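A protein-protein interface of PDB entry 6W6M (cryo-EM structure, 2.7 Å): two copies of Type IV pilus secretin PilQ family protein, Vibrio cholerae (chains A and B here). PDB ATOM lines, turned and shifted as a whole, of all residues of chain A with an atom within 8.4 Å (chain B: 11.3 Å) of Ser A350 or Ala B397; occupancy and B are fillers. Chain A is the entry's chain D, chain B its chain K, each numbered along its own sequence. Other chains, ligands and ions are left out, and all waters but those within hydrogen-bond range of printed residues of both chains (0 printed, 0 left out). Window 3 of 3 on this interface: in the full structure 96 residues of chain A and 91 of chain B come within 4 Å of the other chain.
NE2 of Gln A363 lies within hydrogen-bond range of OD1 of Asn A360 (3.0 Å).
The backbone carbonyl oxygen (O) of Met B345 sits at hydrogen-bond distance from the backbone NH (N) of Leu B404 (2.9 Å).
O of Leu B407 lies within hydrogen-bond range of N of Phe B394 (2.9 Å).
The backbone NH of Val B396 lies within hydrogen-bond range of the backbone carbonyl oxygen of Leu B405 (2.9 Å).
No position is printed for both chains.
O of Ser A350 touches CA of Val B396, at 3.6 Å.
Ala B397 touches Ser A350.
Gln B395 touches Ser A352 (N to O, 3.7 Å).
Ala B393 touches Val A353.
Val A353 touches Phe B394 (CG2 to CD2, 3.98 Å).
Asn A360 touches Phe B394.
O of Asn A360 touches OE1 of Gln B395, at 3.6 Å.
Leu A361 touches Phe B372 (CD1 to CE2, 3.9 Å).
Lys A364 touches Gln B395 (CE to OE1, 3.7 Å).
Leu A366 touches Leu B404 (CD1 to CD1, 3.9 Å).
Of the 22 printed residues of chain B, 7 touch a printed residue of chain A.
Along chain B the printed residues that touch a printed residue of chain A span positions 372 to 404.
Of the 12 printed residues of chain A, 8 touch a printed residue of chain B.
Printed residues of chain A that touch a printed residue of chain B: Ser A350, His A351, Ser A352, Val A353, Asn A360, Leu A361, Lys A364 and Leu A366.
Hydrophobic or aromatic side chains of chain A that line the printed part of chain B: Val A353, Leu A361 and Leu A366.
Among the printed residues, 13 pairs touch across the chains.
No residue of chain B comes within 4 Å of Asn A348.
No residue of chain B comes within 4 Å of Gly A349.
Ser A352 touches one residue of chain B.
Printed residues of chain B within 4 Å of Asn A360: Ala B393, Phe B394 and Gln B395.
Printed residues of chain B within 4 Å of Leu A361: Phe B372 and Gln B395.
Of the printed residues of chain B, Lys A364 touches Gln B395.
Of the printed residues of chain A, Val B396 touches Ser A350 (3.6 Å).
Printed residues of chain A within 4 Å of Ala B397: Ser A350 (3.4 Å).
Of the printed residues of chain A, Leu B404 touches Leu A366.
The nearest residue of chain A that does not touch Ala B397 is Lys A364 (4.8 Å).
The nearest printed residue of chain A that does not touch Leu B404 is Leu A361 (4.8 Å).
ND2 of Asn A360 is in hydrogen-bond range of O of Ala B393 (3.2 Å).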
ATOM      1  N   THR A 347     -17.897 -17.841  16.875  1.00  0.00           N
ATOM      2  CA  THR A 347     -19.335 -17.879  17.100  1.00  0.00           C
ATOM      3  C   THR A 347     -20.031 -18.079  15.762  1.00  0.00           C
ATOM      4  O   THR A 347     -19.466 -17.797  14.706  1.00  0.00           O
ATOM      5  CB  THR A 347     -19.847 -16.608  17.789  1.00  0.00           C
ATOM      6  OG1 THR A 347     -19.534 -15.474  16.979  1.00  0.00           O
ATOM      7  CG2 THR A 347     -19.193 -16.433  19.129  1.00  0.00           C
ATOM      8  N   ASN A 348     -21.254 -18.590  15.811  1.00  0.00           N
ATOM      9  CA  ASN A 348     -21.979 -18.942  14.602  1.00  0.00           C
ATOM     10  C   ASN A 348     -23.428 -18.487  14.598  1.00  0.00           C
ATOM     11  O   ASN A 348     -24.082 -18.576  13.557  1.00  0.00           O
ATOM     12  CB  ASN A 348     -21.930 -20.463  14.391  1.00  0.00           C
ATOM     13  CG  ASN A 348     -22.405 -20.877  13.024  1.00  0.00           C
ATOM     14  OD1 ASN A 348     -22.246 -20.142  12.050  1.00  0.00           O
ATOM     15  ND2 ASN A 348     -22.983 -22.068  12.934  1.00  0.00           N
ATOM     16  N   GLY A 349     -23.938 -17.985  15.710  1.00  0.00           N
ATOM     17  CA  GLY A 349     -25.362 -17.827  15.872  1.00  0.00           C
ATOM     18  C   GLY A 349     -25.901 -19.021  16.629  1.00  0.00           C
ATOM     19  O   GLY A 349     -26.075 -20.099  16.053  1.00  0.00           O
ATOM     20  N   SER A 350     -26.144 -18.843  17.927  1.00  0.00           N
ATOM     21  CA  SER A 350     -26.592 -19.914  18.821  1.00  0.00           C
ATOM     22  C   SER A 350     -25.574 -21.048  18.945  1.00  0.00           C
ATOM     23  O   SER A 350     -25.857 -22.070  19.564  1.00  0.00           O
ATOM     24  CB  SER A 350     -27.949 -20.479  18.387  1.00  0.00           C
ATOM     25  OG  SER A 350     -27.802 -21.310  17.250  1.00  0.00           O
ATOM     26  N   HIS A 351     -24.379 -20.881  18.384  1.00  0.00           N
ATOM     27  CA  HIS A 351     -23.323 -21.883  18.473  1.00  0.00           C
ATOM     28  C   HIS A 351     -22.000 -21.166  18.673  1.00  0.00           C
ATOM     29  O   HIS A 351     -21.726 -20.177  17.995  1.00  0.00           O
ATOM     30  CB  HIS A 351     -23.233 -22.748  17.215  1.00  0.00           C
ATOM     31  CG  HIS A 351     -24.287 -23.802  17.116  1.00  0.00           C
ATOM     32  ND1 HIS A 351     -23.993 -25.111  16.805  1.00  0.00           N
ATOM     33  CD2 HIS A 351     -25.630 -23.744  17.264  1.00  0.00           C
ATOM     34  CE1 HIS A 351     -25.110 -25.817  16.776  1.00  0.00           C
ATOM     35  NE2 HIS A 351     -26.118 -25.011  17.052  1.00  0.00           N
ATOM     36  N   SER A 352     -21.173 -21.679  19.580  1.00  0.00           N
ATOM     37  CA  SER A 352     -19.902 -21.041  19.896  1.00  0.00           C
ATOM     38  C   SER A 352     -18.830 -22.087  20.130  1.00  0.00           C
ATOM     39  O   SER A 352     -19.123 -23.263  20.334  1.00  0.00           O
ATOM     40  CB  SER A 352     -20.020 -20.156  21.133  1.00  0.00           C
ATOM     41  OG  SER A 352     -20.891 -19.076  20.887  1.00  0.00           O
ATOM     42  N   VAL A 353     -17.579 -21.644  20.088  1.00  0.00           N
ATOM     43  CA  VAL A 353     -16.429 -22.486  20.389  1.00  0.00           C
ATOM     44  C   VAL A 353     -15.360 -21.627  21.041  1.00  0.00           C
ATOM     45  O   VAL A 353     -15.020 -20.553  20.536  1.00  0.00           O
ATOM     46  CB  VAL A 353     -15.855 -23.177  19.140  1.00  0.00           C
ATOM     47  CG1 VAL A 353     -14.605 -23.925  19.507  1.00  0.00           C
ATOM     48  CG2 VAL A 353     -16.851 -24.140  18.555  1.00  0.00           C
ATOM     49  N   ASN A 360     -17.011 -18.771  26.627  1.00  0.00           N
ATOM     50  CA  ASN A 360     -18.265 -18.797  25.884  1.00  0.00           C
ATOM     51  C   ASN A 360     -19.317 -17.909  26.536  1.00  0.00           C
ATOM     52  O   ASN A 360     -20.185 -17.364  25.851  1.00  0.00           O
ATOM     53  CB  ASN A 360     -18.786 -20.226  25.765  1.00  0.00           C
ATOM     54  CG  ASN A 360     -17.953 -21.075  24.844  1.00  0.00           C
ATOM     55  OD1 ASN A 360     -17.168 -20.569  24.053  1.00  0.00           O
ATOM     56  ND2 ASN A 360     -18.126 -22.379  24.937  1.00  0.00           N
ATOM     57  N   LEU A 361     -19.276 -17.771  27.858  1.00  0.00           N
ATOM     58  CA  LEU A 361     -20.237 -16.883  28.503  1.00  0.00           C
ATOM     59  C   LEU A 361     -19.880 -15.421  28.272  1.00  0.00           C
ATOM     60  O   LEU A 361     -20.740 -14.544  28.382  1.00  0.00           O
ATOM     61  CB  LEU A 361     -20.327 -17.189  29.995  1.00  0.00           C
ATOM     62  CG  LEU A 361     -20.858 -18.572  30.371  1.00  0.00           C
ATOM     63  CD1 LEU A 361     -20.888 -18.733  31.871  1.00  0.00           C
ATOM     64  CD2 LEU A 361     -22.232 -18.793  29.793  1.00  0.00           C
ATOM     65  N   GLN A 363     -18.406 -14.195  25.287  1.00  0.00           N
ATOM     66  CA  GLN A 363     -18.754 -13.831  23.921  1.00  0.00           C
ATOM     67  C   GLN A 363     -20.255 -13.979  23.740  1.00  0.00           C
ATOM     68  O   GLN A 363     -20.730 -14.675  22.839  1.00  0.00           O
ATOM     69  CB  GLN A 363     -17.976 -14.672  22.908  1.00  0.00           C
ATOM     70  CG  GLN A 363     -18.070 -16.159  23.099  1.00  0.00           C
ATOM     71  CD  GLN A 363     -17.342 -16.918  22.022  1.00  0.00           C
ATOM     72  OE1 GLN A 363     -16.768 -16.323  21.117  1.00  0.00           O
ATOM     73  NE2 GLN A 363     -17.363 -18.236  22.109  1.00  0.00           N
ATOM     74  N   LYS A 364     -20.976 -13.321  24.630  1.00  0.00           N
ATOM     75  CA  LYS A 364     -22.433 -13.227  24.673  1.00  0.00           C
ATOM     76  C   LYS A 364     -22.733 -12.077  25.633  1.00  0.00           C
ATOM     77  O   LYS A 364     -21.861 -11.241  25.941  1.00  0.00           O
ATOM     78  CB  LYS A 364     -23.073 -14.498  25.244  1.00  0.00           C
ATOM     79  CG  LYS A 364     -22.817 -15.784  24.475  1.00  0.00           C
ATOM     80  CD  LYS A 364     -23.424 -15.731  23.084  1.00  0.00           C
ATOM     81  CE  LYS A 364     -23.225 -17.047  22.352  1.00  0.00           C
ATOM     82  NZ  LYS A 364     -23.793 -17.005  20.976  1.00  0.00           N
ATOM     83  N   LEU A 366     -23.750 -12.632  28.817  1.00  0.00           N
ATOM     84  CA  LEU A 366     -24.079 -13.253  30.096  1.00  0.00           C
ATOM     85  C   LEU A 366     -23.177 -12.758  31.225  1.00  0.00           C
ATOM     86  O   LEU A 366     -23.664 -12.376  32.294  1.00  0.00           O
ATOM     87  CB  LEU A 366     -24.028 -14.771  29.948  1.00  0.00           C
ATOM     88  CG  LEU A 366     -25.122 -15.231  28.981  1.00  0.00           C
ATOM     89  CD1 LEU A 366     -25.040 -16.705  28.673  1.00  0.00           C
ATOM     90  CD2 LEU A 366     -26.475 -14.900  29.550  1.00  0.00           C
ATOM     91  N   GLY B 343     -23.005 -28.619  31.862  1.00  0.00           N
ATOM     92  CA  GLY B 343     -24.194 -28.096  32.511  1.00  0.00           C
ATOM     93  C   GLY B 343     -25.318 -27.840  31.534  1.00  0.00           C
ATOM     94  O   GLY B 343     -25.094 -27.671  30.331  1.00  0.00           O
ATOM     95  N   VAL B 344     -26.543 -27.806  32.058  1.00  0.00           N
ATOM     96  CA  VAL B 344     -27.736 -27.564  31.263  1.00  0.00           C
ATOM     97  C   VAL B 344     -28.633 -26.585  32.008  1.00  0.00           C
ATOM     98  O   VAL B 344     -28.520 -26.399  33.219  1.00  0.00           O
ATOM     99  CB  VAL B 344     -28.506 -28.861  30.947  1.00  0.00           C
ATOM    100  CG1 VAL B 344     -29.797 -28.556  30.227  1.00  0.00           C
ATOM    101  CG2 VAL B 344     -27.659 -29.783  30.119  1.00  0.00           C
ATOM    102  N   MET B 345     -29.526 -25.941  31.262  1.00  0.00           N
ATOM    103  CA  MET B 345     -30.435 -24.969  31.867  1.00  0.00           C
ATOM    104  C   MET B 345     -31.608 -24.769  30.927  1.00  0.00           C
ATOM    105  O   MET B 345     -31.418 -24.278  29.814  1.00  0.00           O
ATOM    106  CB  MET B 345     -29.704 -23.656  32.116  1.00  0.00           C
ATOM    107  CG  MET B 345     -30.510 -22.597  32.797  1.00  0.00           C
ATOM    108  SD  MET B 345     -29.506 -21.146  33.138  1.00  0.00           S
ATOM    109  CE  MET B 345     -28.591 -21.673  34.573  1.00  0.00           C
ATOM    110  N   SER B 346     -32.811 -25.142  31.348  1.00  0.00           N
ATOM    111  CA  SER B 346     -33.932 -25.064  30.426  1.00  0.00           C
ATOM    112  C   SER B 346     -35.201 -24.688  31.170  1.00  0.00           C
ATOM    113  O   SER B 346     -35.353 -24.964  32.359  1.00  0.00           O
ATOM    114  CB  SER B 346     -34.124 -26.383  29.684  1.00  0.00           C
ATOM    115  OG  SER B 346     -34.468 -27.416  30.583  1.00  0.00           O
ATOM    116  N   TRP B 362     -33.013 -18.819  40.125  1.00  0.00           N
ATOM    117  CA  TRP B 362     -32.482 -17.682  39.380  1.00  0.00           C
ATOM    118  C   TRP B 362     -33.177 -17.511  38.038  1.00  0.00           C
ATOM    119  O   TRP B 362     -33.475 -16.385  37.632  1.00  0.00           O
ATOM    120  CB  TRP B 362     -30.982 -17.829  39.169  1.00  0.00           C
ATOM    121  CG  TRP B 362     -30.402 -16.734  38.337  1.00  0.00           C
ATOM    122  CD1 TRP B 362     -29.912 -15.545  38.778  1.00  0.00           C
ATOM    123  CD2 TRP B 362     -30.247 -16.727  36.915  1.00  0.00           C
ATOM    124  NE1 TRP B 362     -29.457 -14.798  37.723  1.00  0.00           N
ATOM    125  CE2 TRP B 362     -29.654 -15.503  36.566  1.00  0.00           C
ATOM    126  CE3 TRP B 362     -30.551 -17.639  35.904  1.00  0.00           C
ATOM    127  CZ2 TRP B 362     -29.360 -15.165  35.250  1.00  0.00           C
ATOM    128  CZ3 TRP B 362     -30.259 -17.304  34.601  1.00  0.00           C
ATOM    129  CH2 TRP B 362     -29.669 -16.079  34.284  1.00  0.00           C
ATOM    130  N   PHE B 372     -24.554 -14.037  37.143  1.00  0.00           N
ATOM    131  CA  PHE B 372     -24.715 -15.420  36.718  1.00  0.00           C
ATOM    132  C   PHE B 372     -24.226 -16.340  37.828  1.00  0.00           C
ATOM    133  O   PHE B 372     -23.114 -16.158  38.335  1.00  0.00           O
ATOM    134  CB  PHE B 372     -23.971 -15.701  35.411  1.00  0.00           C
ATOM    135  CG  PHE B 372     -24.557 -16.831  34.624  1.00  0.00           C
ATOM    136  CD1 PHE B 372     -25.865 -16.779  34.189  1.00  0.00           C
ATOM    137  CD2 PHE B 372     -23.805 -17.945  34.320  1.00  0.00           C
ATOM    138  CE1 PHE B 372     -26.409 -17.815  33.470  1.00  0.00           C
ATOM    139  CE2 PHE B 372     -24.349 -18.983  33.601  1.00  0.00           C
ATOM    140  CZ  PHE B 372     -25.649 -18.918  33.175  1.00  0.00           C
ATOM    141  N   PHE B 377     -24.658 -23.255  38.274  1.00  0.00           N
ATOM    142  CA  PHE B 377     -25.108 -23.630  36.943  1.00  0.00           C
ATOM    143  C   PHE B 377     -24.748 -25.068  36.607  1.00  0.00           C
ATOM    144  O   PHE B 377     -25.579 -25.794  36.053  1.00  0.00           O
ATOM    145  CB  PHE B 377     -24.514 -22.663  35.914  1.00  0.00           C
ATOM    146  CG  PHE B 377     -24.653 -23.116  34.491  1.00  0.00           C
ATOM    147  CD1 PHE B 377     -25.895 -23.206  33.893  1.00  0.00           C
ATOM    148  CD2 PHE B 377     -23.541 -23.429  33.742  1.00  0.00           C
ATOM    149  CE1 PHE B 377     -26.021 -23.624  32.592  1.00  0.00           C
ATOM    150  CE2 PHE B 377     -23.665 -23.844  32.439  1.00  0.00           C
ATOM    151  CZ  PHE B 377     -24.908 -23.941  31.865  1.00  0.00           C
ATOM    152  N   ALA B 393     -14.158 -26.176  24.851  1.00  0.00           N
ATOM    153  CA  ALA B 393     -15.549 -26.059  25.267  1.00  0.00           C
ATOM    154  C   ALA B 393     -16.583 -25.590  24.255  1.00  0.00           C
ATOM    155  O   ALA B 393     -16.371 -24.608  23.544  1.00  0.00           O
ATOM    156  CB  ALA B 393     -15.608 -25.134  26.473  1.00  0.00           C
ATOM    157  N   PHE B 394     -17.696 -26.309  24.185  1.00  0.00           N
ATOM    158  CA  PHE B 394     -18.751 -26.092  23.208  1.00  0.00           C
ATOM    159  C   PHE B 394     -20.021 -25.628  23.910  1.00  0.00           C
ATOM    160  O   PHE B 394     -20.260 -25.937  25.080  1.00  0.00           O
ATOM    161  CB  PHE B 394     -19.043 -27.362  22.413  1.00  0.00           C
ATOM    162  CG  PHE B 394     -17.826 -27.995  21.807  1.00  0.00           C
ATOM    163  CD1 PHE B 394     -17.227 -29.090  22.405  1.00  0.00           C
ATOM    164  CD2 PHE B 394     -17.283 -27.504  20.635  1.00  0.00           C
ATOM    165  CE1 PHE B 394     -16.114 -29.677  21.849  1.00  0.00           C
ATOM    166  CE2 PHE B 394     -16.170 -28.089  20.075  1.00  0.00           C
ATOM    167  CZ  PHE B 394     -15.586 -29.176  20.684  1.00  0.00           C
ATOM    168  N   GLN B 395     -20.852 -24.899  23.173  1.00  0.00           N
ATOM    169  CA  GLN B 395     -22.027 -24.266  23.756  1.00  0.00           C
ATOM    170  C   GLN B 395     -23.181 -24.283  22.767  1.00  0.00           C
ATOM    171  O   GLN B 395     -22.971 -24.328  21.556  1.00  0.00           O
ATOM    172  CB  GLN B 395     -21.721 -22.830  24.171  1.00  0.00           C
ATOM    173  CG  GLN B 395     -22.788 -22.192  25.007  1.00  0.00           C
ATOM    174  CD  GLN B 395     -22.526 -20.737  25.253  1.00  0.00           C
ATOM    175  OE1 GLN B 395     -22.147 -20.005  24.350  1.00  0.00           O
ATOM    176  NE2 GLN B 395     -22.719 -20.305  26.481  1.00  0.00           N
ATOM    177  N   VAL B 396     -24.401 -24.283  23.297  1.00  0.00           N
ATOM    178  CA  VAL B 396     -25.614 -24.052  22.520  1.00  0.00           C
ATOM    179  C   VAL B 396     -26.528 -23.174  23.358  1.00  0.00           C
ATOM    180  O   VAL B 396     -27.087 -23.636  24.359  1.00  0.00           O
ATOM    181  CB  VAL B 396     -26.326 -25.357  22.141  1.00  0.00           C
ATOM    182  CG1 VAL B 396     -27.703 -25.053  21.618  1.00  0.00           C
ATOM    183  CG2 VAL B 396     -25.542 -26.104  21.098  1.00  0.00           C
ATOM    184  N   ALA B 397     -26.670 -21.913  22.966  1.00  0.00           N
ATOM    185  CA  ALA B 397     -27.447 -20.951  23.735  1.00  0.00           C
ATOM    186  C   ALA B 397     -28.490 -20.320  22.835  1.00  0.00           C
ATOM    187  O   ALA B 397     -28.138 -19.669  21.850  1.00  0.00           O
ATOM    188  CB  ALA B 397     -26.552 -19.864  24.335  1.00  0.00           C
ATOM    189  N   LYS B 398     -29.764 -20.499  23.175  1.00  0.00           N
ATOM    190  CA  LYS B 398     -30.860 -19.889  22.435  1.00  0.00           C
ATOM    191  C   LYS B 398     -31.289 -18.557  23.027  1.00  0.00           C
ATOM    192  O   LYS B 398     -31.285 -17.542  22.327  1.00  0.00           O
ATOM    193  CB  LYS B 398     -32.070 -20.829  22.386  1.00  0.00           C
ATOM    194  CG  LYS B 398     -31.774 -22.224  21.886  1.00  0.00           C
ATOM    195  CD  LYS B 398     -31.733 -22.306  20.381  1.00  0.00           C
ATOM    196  CE  LYS B 398     -31.609 -23.758  19.937  1.00  0.00           C
ATOM    197  NZ  LYS B 398     -31.371 -23.897  18.475  1.00  0.00           N
ATOM    198  N   LEU B 399     -31.673 -18.542  24.302  1.00  0.00           N
ATOM    199  CA  LEU B 399     -32.142 -17.380  25.049  1.00  0.00           C
ATOM    200  C   LEU B 399     -33.484 -16.869  24.540  1.00  0.00           C
ATOM    201  O   LEU B 399     -34.044 -15.941  25.131  1.00  0.00           O
ATOM    202  CB  LEU B 399     -31.123 -16.231  25.048  1.00  0.00           C
ATOM    203  CG  LEU B 399     -29.794 -16.502  25.763  1.00  0.00           C
ATOM    204  CD1 LEU B 399     -28.824 -15.350  25.564  1.00  0.00           C
ATOM    205  CD2 LEU B 399     -30.018 -16.757  27.248  1.00  0.00           C
ATOM    206  N   GLY B 400     -34.023 -17.446  23.470  1.00  0.00           N
ATOM    207  CA  GLY B 400     -35.366 -17.143  23.023  1.00  0.00           C
ATOM    208  C   GLY B 400     -36.341 -18.105  23.657  1.00  0.00           C
ATOM    209  O   GLY B 400     -37.329 -17.686  24.264  1.00  0.00           O
ATOM    210  N   SER B 401     -36.065 -19.405  23.530  1.00  0.00           N
ATOM    211  CA  SER B 401     -36.802 -20.407  24.291  1.00  0.00           C
ATOM    212  C   SER B 401     -36.199 -20.654  25.667  1.00  0.00           C
ATOM    213  O   SER B 401     -36.804 -21.366  26.475  1.00  0.00           O
ATOM    214  CB  SER B 401     -36.870 -21.724  23.516  1.00  0.00           C
ATOM    215  OG  SER B 401     -35.583 -22.277  23.328  1.00  0.00           O
ATOM    216  N   GLY B 402     -35.021 -20.102  25.941  1.00  0.00           N
ATOM    217  CA  GLY B 402     -34.377 -20.198  27.238  1.00  0.00           C
ATOM    218  C   GLY B 402     -33.260 -21.216  27.316  1.00  0.00           C
ATOM    219  O   GLY B 402     -32.336 -21.038  28.121  1.00  0.00           O
ATOM    220  N   THR B 403     -33.297 -22.262  26.495  1.00  0.00           N
ATOM    221  CA  THR B 403     -32.374 -23.378  26.629  1.00  0.00           C
ATOM    222  C   THR B 403     -30.921 -22.925  26.524  1.00  0.00           C
ATOM    223  O   THR B 403     -30.571 -22.070  25.714  1.00  0.00           O
ATOM    224  CB  THR B 403     -32.673 -24.425  25.560  1.00  0.00           C
ATOM    225  OG1 THR B 403     -34.008 -24.910  25.737  1.00  0.00           O
ATOM    226  CG2 THR B 403     -31.698 -25.588  25.642  1.00  0.00           C
ATOM    227  N   LEU B 404     -30.072 -23.519  27.363  1.00  0.00           N
ATOM    228  CA  LEU B 404     -28.630 -23.322  27.321  1.00  0.00           C
ATOM    229  C   LEU B 404     -27.965 -24.637  27.688  1.00  0.00           C
ATOM    230  O   LEU B 404     -28.433 -25.334  28.590  1.00  0.00           O
ATOM    231  CB  LEU B 404     -28.192 -22.213  28.286  1.00  0.00           C
ATOM    232  CG  LEU B 404     -26.742 -21.738  28.244  1.00  0.00           C
ATOM    233  CD1 LEU B 404     -26.670 -20.269  28.573  1.00  0.00           C
ATOM    234  CD2 LEU B 404     -25.885 -22.497  29.209  1.00  0.00           C
ATOM    235  N   LEU B 405     -26.885 -24.975  26.986  1.00  0.00           N
ATOM    236  CA  LEU B 405     -26.130 -26.158  27.373  1.00  0.00           C
ATOM    237  C   LEU B 405     -24.653 -25.969  27.059  1.00  0.00           C
ATOM    238  O   LEU B 405     -24.297 -25.504  25.976  1.00  0.00           O
ATOM    239  CB  LEU B 405     -26.676 -27.417  26.694  1.00  0.00           C
ATOM    240  CG  LEU B 405     -26.180 -28.805  27.068  1.00  0.00           C
ATOM    241  CD1 LEU B 405     -27.294 -29.835  26.940  1.00  0.00           C
ATOM    242  CD2 LEU B 405     -25.001 -29.178  26.186  1.00  0.00           C
ATOM    243  N   ASP B 406     -23.802 -26.347  28.017  1.00  0.00           N
ATOM    244  CA  ASP B 406     -22.354 -26.178  27.941  1.00  0.00           C
ATOM    245  C   ASP B 406     -21.641 -27.501  28.181  1.00  0.00           C
ATOM    246  O   ASP B 406     -22.059 -28.293  29.032  1.00  0.00           O
ATOM    247  CB  ASP B 406     -21.869 -25.181  28.980  1.00  0.00           C
ATOM    248  CG  ASP B 406     -22.264 -23.772  28.665  1.00  0.00           C
ATOM    249  OD1 ASP B 406     -23.228 -23.582  27.904  1.00  0.00           O
ATOM    250  OD2 ASP B 406     -21.600 -22.850  29.164  1.00  0.00           O
ATOM    251  N   LEU B 407     -20.525 -27.709  27.471  1.00  0.00           N
ATOM    252  CA  LEU B 407     -19.726 -28.920  27.638  1.00  0.00           C
ATOM    253  C   LEU B 407     -18.249 -28.628  27.419  1.00  0.00           C
ATOM    254  O   LEU B 407     -17.870 -28.219  26.324  1.00  0.00           O
ATOM    255  CB  LEU B 407     -20.176 -30.011  26.664  1.00  0.00           C
ATOM    256  CG  LEU B 407     -19.396 -31.327  26.656  1.00  0.00           C
ATOM    257  CD1 LEU B 407     -19.502 -32.033  27.983  1.00  0.00           C
ATOM    258  CD2 LEU B 407     -19.892 -32.235  25.557  1.00  0.00           C
